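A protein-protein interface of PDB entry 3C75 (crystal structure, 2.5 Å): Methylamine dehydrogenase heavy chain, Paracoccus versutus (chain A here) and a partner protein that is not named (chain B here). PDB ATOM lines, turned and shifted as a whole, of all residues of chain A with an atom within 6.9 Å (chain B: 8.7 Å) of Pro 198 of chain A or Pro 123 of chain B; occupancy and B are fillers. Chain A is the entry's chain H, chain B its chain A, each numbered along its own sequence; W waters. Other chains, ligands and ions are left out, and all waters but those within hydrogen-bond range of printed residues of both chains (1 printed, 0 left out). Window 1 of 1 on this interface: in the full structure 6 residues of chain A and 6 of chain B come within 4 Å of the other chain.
The backbone carbonyl oxygen (O) of Pro 198 of chain A lies within hydrogen-bond range of the side-chain amino group (NZ) of Lys 85 of chain B (3.5 Å).
The side-chain carboxylate (OD2) of Asp 220 of chain A lies within salt-bridge range of the guanidinium group (NH1) of Arg 126 of chain B.
The backbone carbonyl oxygen of Ala 199 of chain A lies close to the side-chain amide oxygen of Gln 195 of chain A (3.1 Å).
The backbone carbonyl oxygen (O) of Phe 118 of chain B lies close to the side-chain hydroxyl (OH) of Tyr 57 of chain B (3.4 Å).
N of Phe 118 of chain B is in hydrogen-bond range of O of Ala 83 of chain B (2.9 Å).
Among the printed residues, pairs that only touch across the chains: Asp 220 of chain A with Phe 124 of chain B (3.2 Å), Ala 199 of chain A with Lys 85 of chain B (3.3 Å), Phe 196 of chain A with Pro 123 of chain B (3.4 Å), Phe 196 of chain A with Pro 121 of chain B (3.5 Å), Pro 198 of chain A with Phe 118 of chain B (3.7 Å), Pro 198 of chain A with Pro 123 of chain B (3.7 Å) and Pro 200 of chain A with Arg 126 of chain B (3.8 Å).
No residue of chain B comes within 4 Å of Ser 197 of chain A.
Of chain B, only Lys 85, Phe 118 and Pro 123 come within 4 Å of Pro 198 of chain A.
Ala 199 of chain A touches just one residue of chain B: Lys 85.
Tyr 57 of chain B touches none of the printed residues of chain A.
Of the printed residues of chain A, Phe 118 of chain B touches Pro 198.
Of the printed residues of chain A, Pro 121 of chain B touches Phe 196 (3.5 Å).
Pro 123 of chain B touches two residues of chain A.
Of the printed residues of chain A, Arg 126 of chain B touches Pro 200 (3.8 Å) and Asp 220 (2.3 Å).
Hydrophobic or aromatic side chains of chain A within 4 Å of the printed part of chain B: Phe 196, Pro 198, Ala 199 and Pro 200.
Hydrophobic or aromatic side chains of chain B that line the printed part of chain A: Phe 118, Pro 123 and Phe 124.
Among the printed residues, Asp or Glu carboxylates within 4 Å of a Lys or Arg side-chain nitrogen of the other chain: Asp 220 of chain A with Arg 126 of chain B (2.3 Å).
Water W1 lies within hydrogen-bond range of the backbone carbonyl oxygen (O) of Pro 198 of chain A (2.7 Å) and the backbone carbonyl oxygen (O) of Pro 123 of chain B (2.8 Å).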
ATOM      1  N   TYR A 194       0.759 -11.067  20.820  1.00  0.00           N
ATOM      2  CA  TYR A 194      -0.690 -11.141  20.661  1.00  0.00           C
ATOM      3  C   TYR A 194      -1.457 -11.432  21.939  1.00  0.00           C
ATOM      4  O   TYR A 194      -1.023 -12.243  22.791  1.00  0.00           O
ATOM      5  CB  TYR A 194      -1.036 -12.276  19.699  1.00  0.00           C
ATOM      6  CG  TYR A 194      -2.507 -12.400  19.365  1.00  0.00           C
ATOM      7  CD1 TYR A 194      -3.117 -11.477  18.520  1.00  0.00           C
ATOM      8  CD2 TYR A 194      -3.262 -13.480  19.807  1.00  0.00           C
ATOM      9  CE1 TYR A 194      -4.437 -11.628  18.101  1.00  0.00           C
ATOM     10  CE2 TYR A 194      -4.597 -13.650  19.398  1.00  0.00           C
ATOM     11  CZ  TYR A 194      -5.181 -12.718  18.533  1.00  0.00           C
ATOM     12  OH  TYR A 194      -6.477 -12.860  18.048  1.00  0.00           O
ATOM     13  N   GLN A 195      -2.621 -10.788  22.045  1.00  0.00           N
ATOM     14  CA  GLN A 195      -3.545 -11.018  23.153  1.00  0.00           C
ATOM     15  C   GLN A 195      -4.755 -11.669  22.473  1.00  0.00           C
ATOM     16  O   GLN A 195      -5.158 -11.240  21.386  1.00  0.00           O
ATOM     17  CB  GLN A 195      -3.985  -9.712  23.803  1.00  0.00           C
ATOM     18  CG  GLN A 195      -4.976  -9.930  24.944  1.00  0.00           C
ATOM     19  CD  GLN A 195      -5.559  -8.647  25.506  1.00  0.00           C
ATOM     20  OE1 GLN A 195      -6.314  -7.958  24.832  1.00  0.00           O
ATOM     21  NE2 GLN A 195      -5.213  -8.325  26.748  1.00  0.00           N
ATOM     22  N   PHE A 196      -5.304 -12.715  23.082  1.00  0.00           N
ATOM     23  CA  PHE A 196      -6.463 -13.388  22.496  1.00  0.00           C
ATOM     24  C   PHE A 196      -7.771 -12.929  23.168  1.00  0.00           C
ATOM     25  O   PHE A 196      -8.657 -12.420  22.487  1.00  0.00           O
ATOM     26  CB  PHE A 196      -6.314 -14.905  22.601  1.00  0.00           C
ATOM     27  CG  PHE A 196      -7.548 -15.668  22.190  1.00  0.00           C
ATOM     28  CD1 PHE A 196      -7.853 -15.864  20.845  1.00  0.00           C
ATOM     29  CD2 PHE A 196      -8.392 -16.225  23.144  1.00  0.00           C
ATOM     30  CE1 PHE A 196      -8.976 -16.612  20.464  1.00  0.00           C
ATOM     31  CE2 PHE A 196      -9.516 -16.975  22.764  1.00  0.00           C
ATOM     32  CZ  PHE A 196      -9.803 -17.167  21.431  1.00  0.00           C
ATOM     33  N   SER A 197      -7.879 -13.135  24.486  1.00  0.00           N
ATOM     34  CA  SER A 197      -9.045 -12.713  25.283  1.00  0.00           C
ATOM     35  C   SER A 197      -8.586 -11.490  26.074  1.00  0.00           C
ATOM     36  O   SER A 197      -7.423 -11.401  26.440  1.00  0.00           O
ATOM     37  CB  SER A 197      -9.457 -13.813  26.282  1.00  0.00           C
ATOM     38  OG  SER A 197     -10.614 -13.468  27.038  1.00  0.00           O
ATOM     39  N   PRO A 198      -9.488 -10.542  26.373  1.00  0.00           N
ATOM     40  CA  PRO A 198     -10.918 -10.451  26.064  1.00  0.00           C
ATOM     41  C   PRO A 198     -11.189 -10.109  24.602  1.00  0.00           C
ATOM     42  O   PRO A 198     -12.288 -10.340  24.078  1.00  0.00           O
ATOM     43  CB  PRO A 198     -11.399  -9.370  27.024  1.00  0.00           C
ATOM     44  CG  PRO A 198     -10.201  -8.462  27.121  1.00  0.00           C
ATOM     45  CD  PRO A 198      -9.086  -9.458  27.283  1.00  0.00           C
ATOM     46  N   ALA A 199     -10.185  -9.563  23.935  1.00  0.00           N
ATOM     47  CA  ALA A 199     -10.362  -9.197  22.534  1.00  0.00           C
ATOM     48  C   ALA A 199      -9.019  -9.173  21.825  1.00  0.00           C
ATOM     49  O   ALA A 199      -7.982  -8.975  22.441  1.00  0.00           O
ATOM     50  CB  ALA A 199     -11.037  -7.842  22.431  1.00  0.00           C
ATOM     51  N   PRO A 200      -9.024  -9.387  20.511  1.00  0.00           N
ATOM     52  CA  PRO A 200      -7.790  -9.394  19.710  1.00  0.00           C
ATOM     53  C   PRO A 200      -7.016  -8.098  19.915  1.00  0.00           C
ATOM     54  O   PRO A 200      -7.608  -7.019  19.854  1.00  0.00           O
ATOM     55  CB  PRO A 200      -8.296  -9.491  18.286  1.00  0.00           C
ATOM     56  CG  PRO A 200      -9.681 -10.097  18.437  1.00  0.00           C
ATOM     57  CD  PRO A 200     -10.222  -9.464  19.666  1.00  0.00           C
ATOM     58  N   ASP A 220     -10.204  -9.820  14.086  1.00  0.00           N
ATOM     59  CA  ASP A 220     -10.110 -11.240  14.455  1.00  0.00           C
ATOM     60  C   ASP A 220      -9.063 -11.896  13.532  1.00  0.00           C
ATOM     61  O   ASP A 220      -9.408 -12.558  12.553  1.00  0.00           O
ATOM     62  CB  ASP A 220     -11.484 -11.924  14.315  1.00  0.00           C
ATOM     63  CG  ASP A 220     -12.601 -11.163  15.068  1.00  0.00           C
ATOM     64  OD1 ASP A 220     -12.426 -10.897  16.266  1.00  0.00           O
ATOM     65  OD2 ASP A 220     -13.649 -10.831  14.472  1.00  0.00           O
ATOM     66  N   TYR A 222      -4.723 -13.596  13.627  1.00  0.00           N
ATOM     67  CA  TYR A 222      -3.703 -14.237  14.462  1.00  0.00           C
ATOM     68  C   TYR A 222      -2.333 -14.236  13.795  1.00  0.00           C
ATOM     69  O   TYR A 222      -2.249 -14.134  12.557  1.00  0.00           O
ATOM     70  CB  TYR A 222      -4.171 -15.641  14.792  1.00  0.00           C
ATOM     71  CG  TYR A 222      -5.628 -15.625  15.160  1.00  0.00           C
ATOM     72  CD1 TYR A 222      -6.593 -15.434  14.191  1.00  0.00           C
ATOM     73  CD2 TYR A 222      -6.041 -15.732  16.478  1.00  0.00           C
ATOM     74  CE1 TYR A 222      -7.940 -15.334  14.516  1.00  0.00           C
ATOM     75  CE2 TYR A 222      -7.391 -15.645  16.812  1.00  0.00           C
ATOM     76  CZ  TYR A 222      -8.334 -15.438  15.816  1.00  0.00           C
ATOM     77  OH  TYR A 222      -9.668 -15.306  16.106  1.00  0.00           O
ATOM     78  N   MET B  55     -22.050 -19.370  14.866  1.00  0.00           N
ATOM     79  CA  MET B  55     -20.967 -18.621  15.503  1.00  0.00           C
ATOM     80  C   MET B  55     -21.161 -17.120  15.542  1.00  0.00           C
ATOM     81  O   MET B  55     -20.189 -16.367  15.535  1.00  0.00           O
ATOM     82  CB  MET B  55     -19.640 -18.941  14.813  1.00  0.00           C
ATOM     83  CG  MET B  55     -19.296 -20.421  14.814  1.00  0.00           C
ATOM     84  SD  MET B  55     -19.248 -21.115  16.510  1.00  0.00           S
ATOM     85  CE  MET B  55     -18.014 -20.060  17.261  1.00  0.00           C
ATOM     86  N   TYR B  57     -24.018 -13.765  16.992  1.00  0.00           N
ATOM     87  CA  TYR B  57     -25.202 -13.263  17.689  1.00  0.00           C
ATOM     88  C   TYR B  57     -25.987 -12.745  16.471  1.00  0.00           C
ATOM     89  O   TYR B  57     -25.598 -11.743  15.863  1.00  0.00           O
ATOM     90  CB  TYR B  57     -24.862 -12.077  18.594  1.00  0.00           C
ATOM     91  CG  TYR B  57     -24.012 -12.429  19.797  1.00  0.00           C
ATOM     92  CD1 TYR B  57     -24.579 -13.010  20.938  1.00  0.00           C
ATOM     93  CD2 TYR B  57     -22.624 -12.228  19.775  1.00  0.00           C
ATOM     94  CE1 TYR B  57     -23.783 -13.384  22.015  1.00  0.00           C
ATOM     95  CE2 TYR B  57     -21.824 -12.605  20.849  1.00  0.00           C
ATOM     96  CZ  TYR B  57     -22.408 -13.183  21.951  1.00  0.00           C
ATOM     97  OH  TYR B  57     -21.610 -13.637  22.950  1.00  0.00           O
ATOM     98  N   HIS B  80     -21.940 -21.191  24.064  1.00  0.00           N
ATOM     99  CA  HIS B  80     -21.776 -19.750  23.894  1.00  0.00           C
ATOM    100  C   HIS B  80     -22.328 -19.060  25.120  1.00  0.00           C
ATOM    101  O   HIS B  80     -23.099 -19.641  25.873  1.00  0.00           O
ATOM    102  CB  HIS B  80     -22.572 -19.249  22.692  1.00  0.00           C
ATOM    103  CG  HIS B  80     -22.086 -19.742  21.362  1.00  0.00           C
ATOM    104  ND1 HIS B  80     -20.848 -19.414  20.853  1.00  0.00           N
ATOM    105  CD2 HIS B  80     -22.727 -20.418  20.379  1.00  0.00           C
ATOM    106  CE1 HIS B  80     -20.753 -19.854  19.613  1.00  0.00           C
ATOM    107  NE2 HIS B  80     -21.880 -20.465  19.299  1.00  0.00           N
ATOM    108  N   ASN B  81     -21.954 -17.804  25.294  1.00  0.00           N
ATOM    109  CA  ASN B  81     -22.434 -17.016  26.425  1.00  0.00           C
ATOM    110  C   ASN B  81     -22.316 -15.510  26.153  1.00  0.00           C
ATOM    111  O   ASN B  81     -21.894 -15.091  25.075  1.00  0.00           O
ATOM    112  CB  ASN B  81     -21.601 -17.352  27.649  1.00  0.00           C
ATOM    113  CG  ASN B  81     -20.262 -16.636  27.644  1.00  0.00           C
ATOM    114  OD1 ASN B  81     -19.661 -16.427  26.581  1.00  0.00           O
ATOM    115  ND2 ASN B  81     -19.780 -16.267  28.833  1.00  0.00           N
ATOM    116  N   ALA B  83     -20.645 -11.979  27.727  1.00  0.00           N
ATOM    117  CA  ALA B  83     -19.596 -11.506  28.611  1.00  0.00           C
ATOM    118  C   ALA B  83     -19.278 -10.031  28.367  1.00  0.00           C
ATOM    119  O   ALA B  83     -19.493  -9.486  27.263  1.00  0.00           O
ATOM    120  CB  ALA B  83     -18.343 -12.339  28.388  1.00  0.00           C
ATOM    121  N   PHE B  84     -18.763  -9.377  29.398  1.00  0.00           N
ATOM    122  CA  PHE B  84     -18.377  -7.980  29.265  1.00  0.00           C
ATOM    123  C   PHE B  84     -16.970  -7.827  29.880  1.00  0.00           C
ATOM    124  O   PHE B  84     -16.604  -8.552  30.811  1.00  0.00           O
ATOM    125  CB  PHE B  84     -19.360  -7.048  30.011  1.00  0.00           C
ATOM    126  CG  PHE B  84     -20.812  -7.182  29.594  1.00  0.00           C
ATOM    127  CD1 PHE B  84     -21.360  -6.355  28.605  1.00  0.00           C
ATOM    128  CD2 PHE B  84     -21.642  -8.119  30.212  1.00  0.00           C
ATOM    129  CE1 PHE B  84     -22.712  -6.460  28.245  1.00  0.00           C
ATOM    130  CE2 PHE B  84     -22.994  -8.232  29.856  1.00  0.00           C
ATOM    131  CZ  PHE B  84     -23.527  -7.403  28.874  1.00  0.00           C
ATOM    132  N   LYS B  85     -16.175  -6.905  29.336  1.00  0.00           N
ATOM    133  CA  LYS B  85     -14.842  -6.623  29.882  1.00  0.00           C
ATOM    134  C   LYS B  85     -15.076  -5.791  31.135  1.00  0.00           C
ATOM    135  O   LYS B  85     -16.194  -5.338  31.398  1.00  0.00           O
ATOM    136  CB  LYS B  85     -13.998  -5.791  28.910  1.00  0.00           C
ATOM    137  CG  LYS B  85     -13.885  -6.373  27.534  1.00  0.00           C
ATOM    138  CD  LYS B  85     -13.302  -5.343  26.568  1.00  0.00           C
ATOM    139  CE  LYS B  85     -13.636  -5.688  25.118  1.00  0.00           C
ATOM    140  NZ  LYS B  85     -13.200  -7.073  24.779  1.00  0.00           N
ATOM    141  N   LYS B  86     -14.025  -5.569  31.905  1.00  0.00           N
ATOM    142  CA  LYS B  86     -14.204  -4.759  33.098  1.00  0.00           C
ATOM    143  C   LYS B  86     -14.518  -3.296  32.772  1.00  0.00           C
ATOM    144  O   LYS B  86     -14.039  -2.748  31.785  1.00  0.00           O
ATOM    145  CB  LYS B  86     -12.971  -4.849  34.003  1.00  0.00           C
ATOM    146  CG  LYS B  86     -11.679  -4.297  33.450  1.00  0.00           C
ATOM    147  CD  LYS B  86     -10.880  -3.698  34.617  1.00  0.00           C
ATOM    148  CE  LYS B  86     -10.910  -4.613  35.883  1.00  0.00           C
ATOM    149  NZ  LYS B  86     -10.727  -3.883  37.197  1.00  0.00           N
ATOM    150  N   ALA B  93     -15.323  -7.045  35.757  1.00  0.00           N
ATOM    151  CA  ALA B  93     -15.721  -7.678  34.498  1.00  0.00           C
ATOM    152  C   ALA B  93     -16.868  -8.680  34.772  1.00  0.00           C
ATOM    153  O   ALA B  93     -16.935  -9.244  35.863  1.00  0.00           O
ATOM    154  CB  ALA B  93     -14.517  -8.400  33.878  1.00  0.00           C
ATOM    155  N   TYR B 117     -20.523  -6.287  24.274  1.00  0.00           N
ATOM    156  CA  TYR B 117     -20.305  -7.615  24.872  1.00  0.00           C
ATOM    157  C   TYR B 117     -19.682  -8.578  23.883  1.00  0.00           C
ATOM    158  O   TYR B 117     -19.593  -8.278  22.704  1.00  0.00           O
ATOM    159  CB  TYR B 117     -21.632  -8.188  25.407  1.00  0.00           C
ATOM    160  CG  TYR B 117     -22.656  -8.557  24.352  1.00  0.00           C
ATOM    161  CD1 TYR B 117     -22.565  -9.769  23.649  1.00  0.00           C
ATOM    162  CD2 TYR B 117     -23.724  -7.712  24.056  1.00  0.00           C
ATOM    163  CE1 TYR B 117     -23.515 -10.131  22.671  1.00  0.00           C
ATOM    164  CE2 TYR B 117     -24.685  -8.067  23.077  1.00  0.00           C
ATOM    165  CZ  TYR B 117     -24.564  -9.279  22.398  1.00  0.00           C
ATOM    166  OH  TYR B 117     -25.500  -9.629  21.466  1.00  0.00           O
ATOM    167  N   PHE B 118     -19.259  -9.738  24.362  1.00  0.00           N
ATOM    168  CA  PHE B 118     -18.625 -10.736  23.490  1.00  0.00           C
ATOM    169  C   PHE B 118     -18.813 -12.130  24.042  1.00  0.00           C
ATOM    170  O   PHE B 118     -19.391 -12.327  25.107  1.00  0.00           O
ATOM    171  CB  PHE B 118     -17.102 -10.484  23.349  1.00  0.00           C
ATOM    172  CG  PHE B 118     -16.345 -10.502  24.662  1.00  0.00           C
ATOM    173  CD1 PHE B 118     -16.448  -9.433  25.568  1.00  0.00           C
ATOM    174  CD2 PHE B 118     -15.594 -11.620  25.030  1.00  0.00           C
ATOM    175  CE1 PHE B 118     -15.817  -9.502  26.824  1.00  0.00           C
ATOM    176  CE2 PHE B 118     -14.962 -11.696  26.274  1.00  0.00           C
ATOM    177  CZ  PHE B 118     -15.076 -10.644  27.169  1.00  0.00           C
ATOM    178  N   CYS B 119     -18.314 -13.113  23.316  1.00  0.00           N
ATOM    179  CA  CYS B 119     -18.443 -14.462  23.802  1.00  0.00           C
ATOM    180  C   CYS B 119     -17.115 -14.787  24.472  1.00  0.00           C
ATOM    181  O   CYS B 119     -16.047 -14.479  23.912  1.00  0.00           O
ATOM    182  CB  CYS B 119     -18.744 -15.419  22.663  1.00  0.00           C
ATOM    183  SG  CYS B 119     -19.053 -17.049  23.284  1.00  0.00           S
ATOM    184  N   THR B 120     -17.172 -15.390  25.669  1.00  0.00           N
ATOM    185  CA  THR B 120     -15.953 -15.696  26.431  1.00  0.00           C
ATOM    186  C   THR B 120     -14.865 -16.434  25.679  1.00  0.00           C
ATOM    187  O   THR B 120     -13.774 -15.908  25.502  1.00  0.00           O
ATOM    188  CB  THR B 120     -16.265 -16.460  27.704  1.00  0.00           C
ATOM    189  OG1 THR B 120     -16.868 -15.566  28.656  1.00  0.00           O
ATOM    190  CG2 THR B 120     -14.992 -17.045  28.271  1.00  0.00           C
ATOM    191  N   PRO B 121     -15.143 -17.657  25.227  1.00  0.00           N
ATOM    192  CA  PRO B 121     -14.145 -18.426  24.488  1.00  0.00           C
ATOM    193  C   PRO B 121     -14.043 -17.959  23.025  1.00  0.00           C
ATOM    194  O   PRO B 121     -13.050 -18.196  22.345  1.00  0.00           O
ATOM    195  CB  PRO B 121     -14.685 -19.836  24.607  1.00  0.00           C
ATOM    196  CG  PRO B 121     -16.167 -19.598  24.480  1.00  0.00           C
ATOM    197  CD  PRO B 121     -16.380 -18.439  25.404  1.00  0.00           C
ATOM    198  N   HIS B 122     -15.082 -17.279  22.549  1.00  0.00           N
ATOM    199  CA  HIS B 122     -15.127 -16.810  21.172  1.00  0.00           C
ATOM    200  C   HIS B 122     -15.100 -15.251  21.099  1.00  0.00           C
ATOM    201  O   HIS B 122     -16.127 -14.614  20.872  1.00  0.00           O
ATOM    202  CB  HIS B 122     -16.394 -17.404  20.546  1.00  0.00           C
ATOM    203  CG  HIS B 122     -16.509 -18.903  20.698  1.00  0.00           C
ATOM    204  ND1 HIS B 122     -17.715 -19.547  20.884  1.00  0.00           N
ATOM    205  CD2 HIS B 122     -15.573 -19.879  20.681  1.00  0.00           C
ATOM    206  CE1 HIS B 122     -17.518 -20.848  20.980  1.00  0.00           C
ATOM    207  NE2 HIS B 122     -16.228 -21.075  20.861  1.00  0.00           N
ATOM    208  N   PRO B 123     -13.906 -14.626  21.287  1.00  0.00           N
ATOM    209  CA  PRO B 123     -13.693 -13.157  21.269  1.00  0.00           C
ATOM    210  C   PRO B 123     -14.099 -12.497  19.954  1.00  0.00           C
ATOM    211  O   PRO B 123     -14.323 -11.290  19.892  1.00  0.00           O
ATOM    212  CB  PRO B 123     -12.186 -12.994  21.521  1.00  0.00           C
ATOM    213  CG  PRO B 123     -11.760 -14.313  22.098  1.00  0.00           C
ATOM    214  CD  PRO B 123     -12.611 -15.329  21.364  1.00  0.00           C
ATOM    215  N   PHE B 124     -14.183 -13.306  18.903  1.00  0.00           N
ATOM    216  CA  PHE B 124     -14.566 -12.813  17.590  1.00  0.00           C
ATOM    217  C   PHE B 124     -16.088 -12.673  17.498  1.00  0.00           C
ATOM    218  O   PHE B 124     -16.614 -12.350  16.464  1.00  0.00           O
ATOM    219  CB  PHE B 124     -14.035 -13.764  16.517  1.00  0.00           C
ATOM    220  CG  PHE B 124     -14.413 -15.195  16.743  1.00  0.00           C
ATOM    221  CD1 PHE B 124     -15.695 -15.652  16.422  1.00  0.00           C
ATOM    222  CD2 PHE B 124     -13.505 -16.080  17.327  1.00  0.00           C
ATOM    223  CE1 PHE B 124     -16.072 -16.964  16.678  1.00  0.00           C
ATOM    224  CE2 PHE B 124     -13.864 -17.398  17.590  1.00  0.00           C
ATOM    225  CZ  PHE B 124     -15.151 -17.843  17.267  1.00  0.00           C
ATOM    226  N   MET B 125     -16.794 -12.920  18.591  1.00  0.00           N
ATOM    227  CA  MET B 125     -18.251 -12.804  18.606  1.00  0.00           C
ATOM    228  C   MET B 125     -18.640 -11.621  19.464  1.00  0.00           C
ATOM    229  O   MET B 125     -18.455 -11.659  20.685  1.00  0.00           O
ATOM    230  CB  MET B 125     -18.875 -14.058  19.197  1.00  0.00           C
ATOM    231  CG  MET B 125     -18.874 -15.228  18.265  1.00  0.00           C
ATOM    232  SD  MET B 125     -19.436 -16.689  19.130  1.00  0.00           S
ATOM    233  CE  MET B 125     -21.219 -16.295  19.374  1.00  0.00           C
ATOM    234  N   ARG B 126     -19.187 -10.575  18.856  1.00  0.00           N
ATOM    235  CA  ARG B 126     -19.563  -9.408  19.644  1.00  0.00           C
ATOM    236  C   ARG B 126     -20.956  -8.918  19.278  1.00  0.00           C
ATOM    237  O   ARG B 126     -21.496  -9.260  18.236  1.00  0.00           O
ATOM    238  CB  ARG B 126     -18.561  -8.271  19.438  1.00  0.00           C
ATOM    239  CG  ARG B 126     -17.140  -8.703  19.420  1.00  0.00           C
ATOM    240  CD  ARG B 126     -16.264  -7.567  18.966  1.00  0.00           C
ATOM    241  NE  ARG B 126     -14.894  -7.993  18.666  1.00  0.00           N
ATOM    242  CZ  ARG B 126     -14.536  -8.689  17.587  1.00  0.00           C
ATOM    243  NH1 ARG B 126     -15.439  -9.049  16.680  1.00  0.00           N
ATOM    244  NH2 ARG B 126     -13.267  -9.027  17.409  1.00  0.00           N
ATOM    245  N   GLY B 127     -21.527  -8.115  20.159  1.00  0.00           N
ATOM    246  CA  GLY B 127     -22.841  -7.569  19.915  1.00  0.00           C
ATOM    247  C   GLY B 127     -22.998  -6.448  20.905  1.00  0.00           C
ATOM    248  O   GLY B 127     -22.073  -6.174  21.664  1.00  0.00           O
HETATM  249  O   HOH W   1     -13.806  -9.482  22.024  1.00  0.00           O
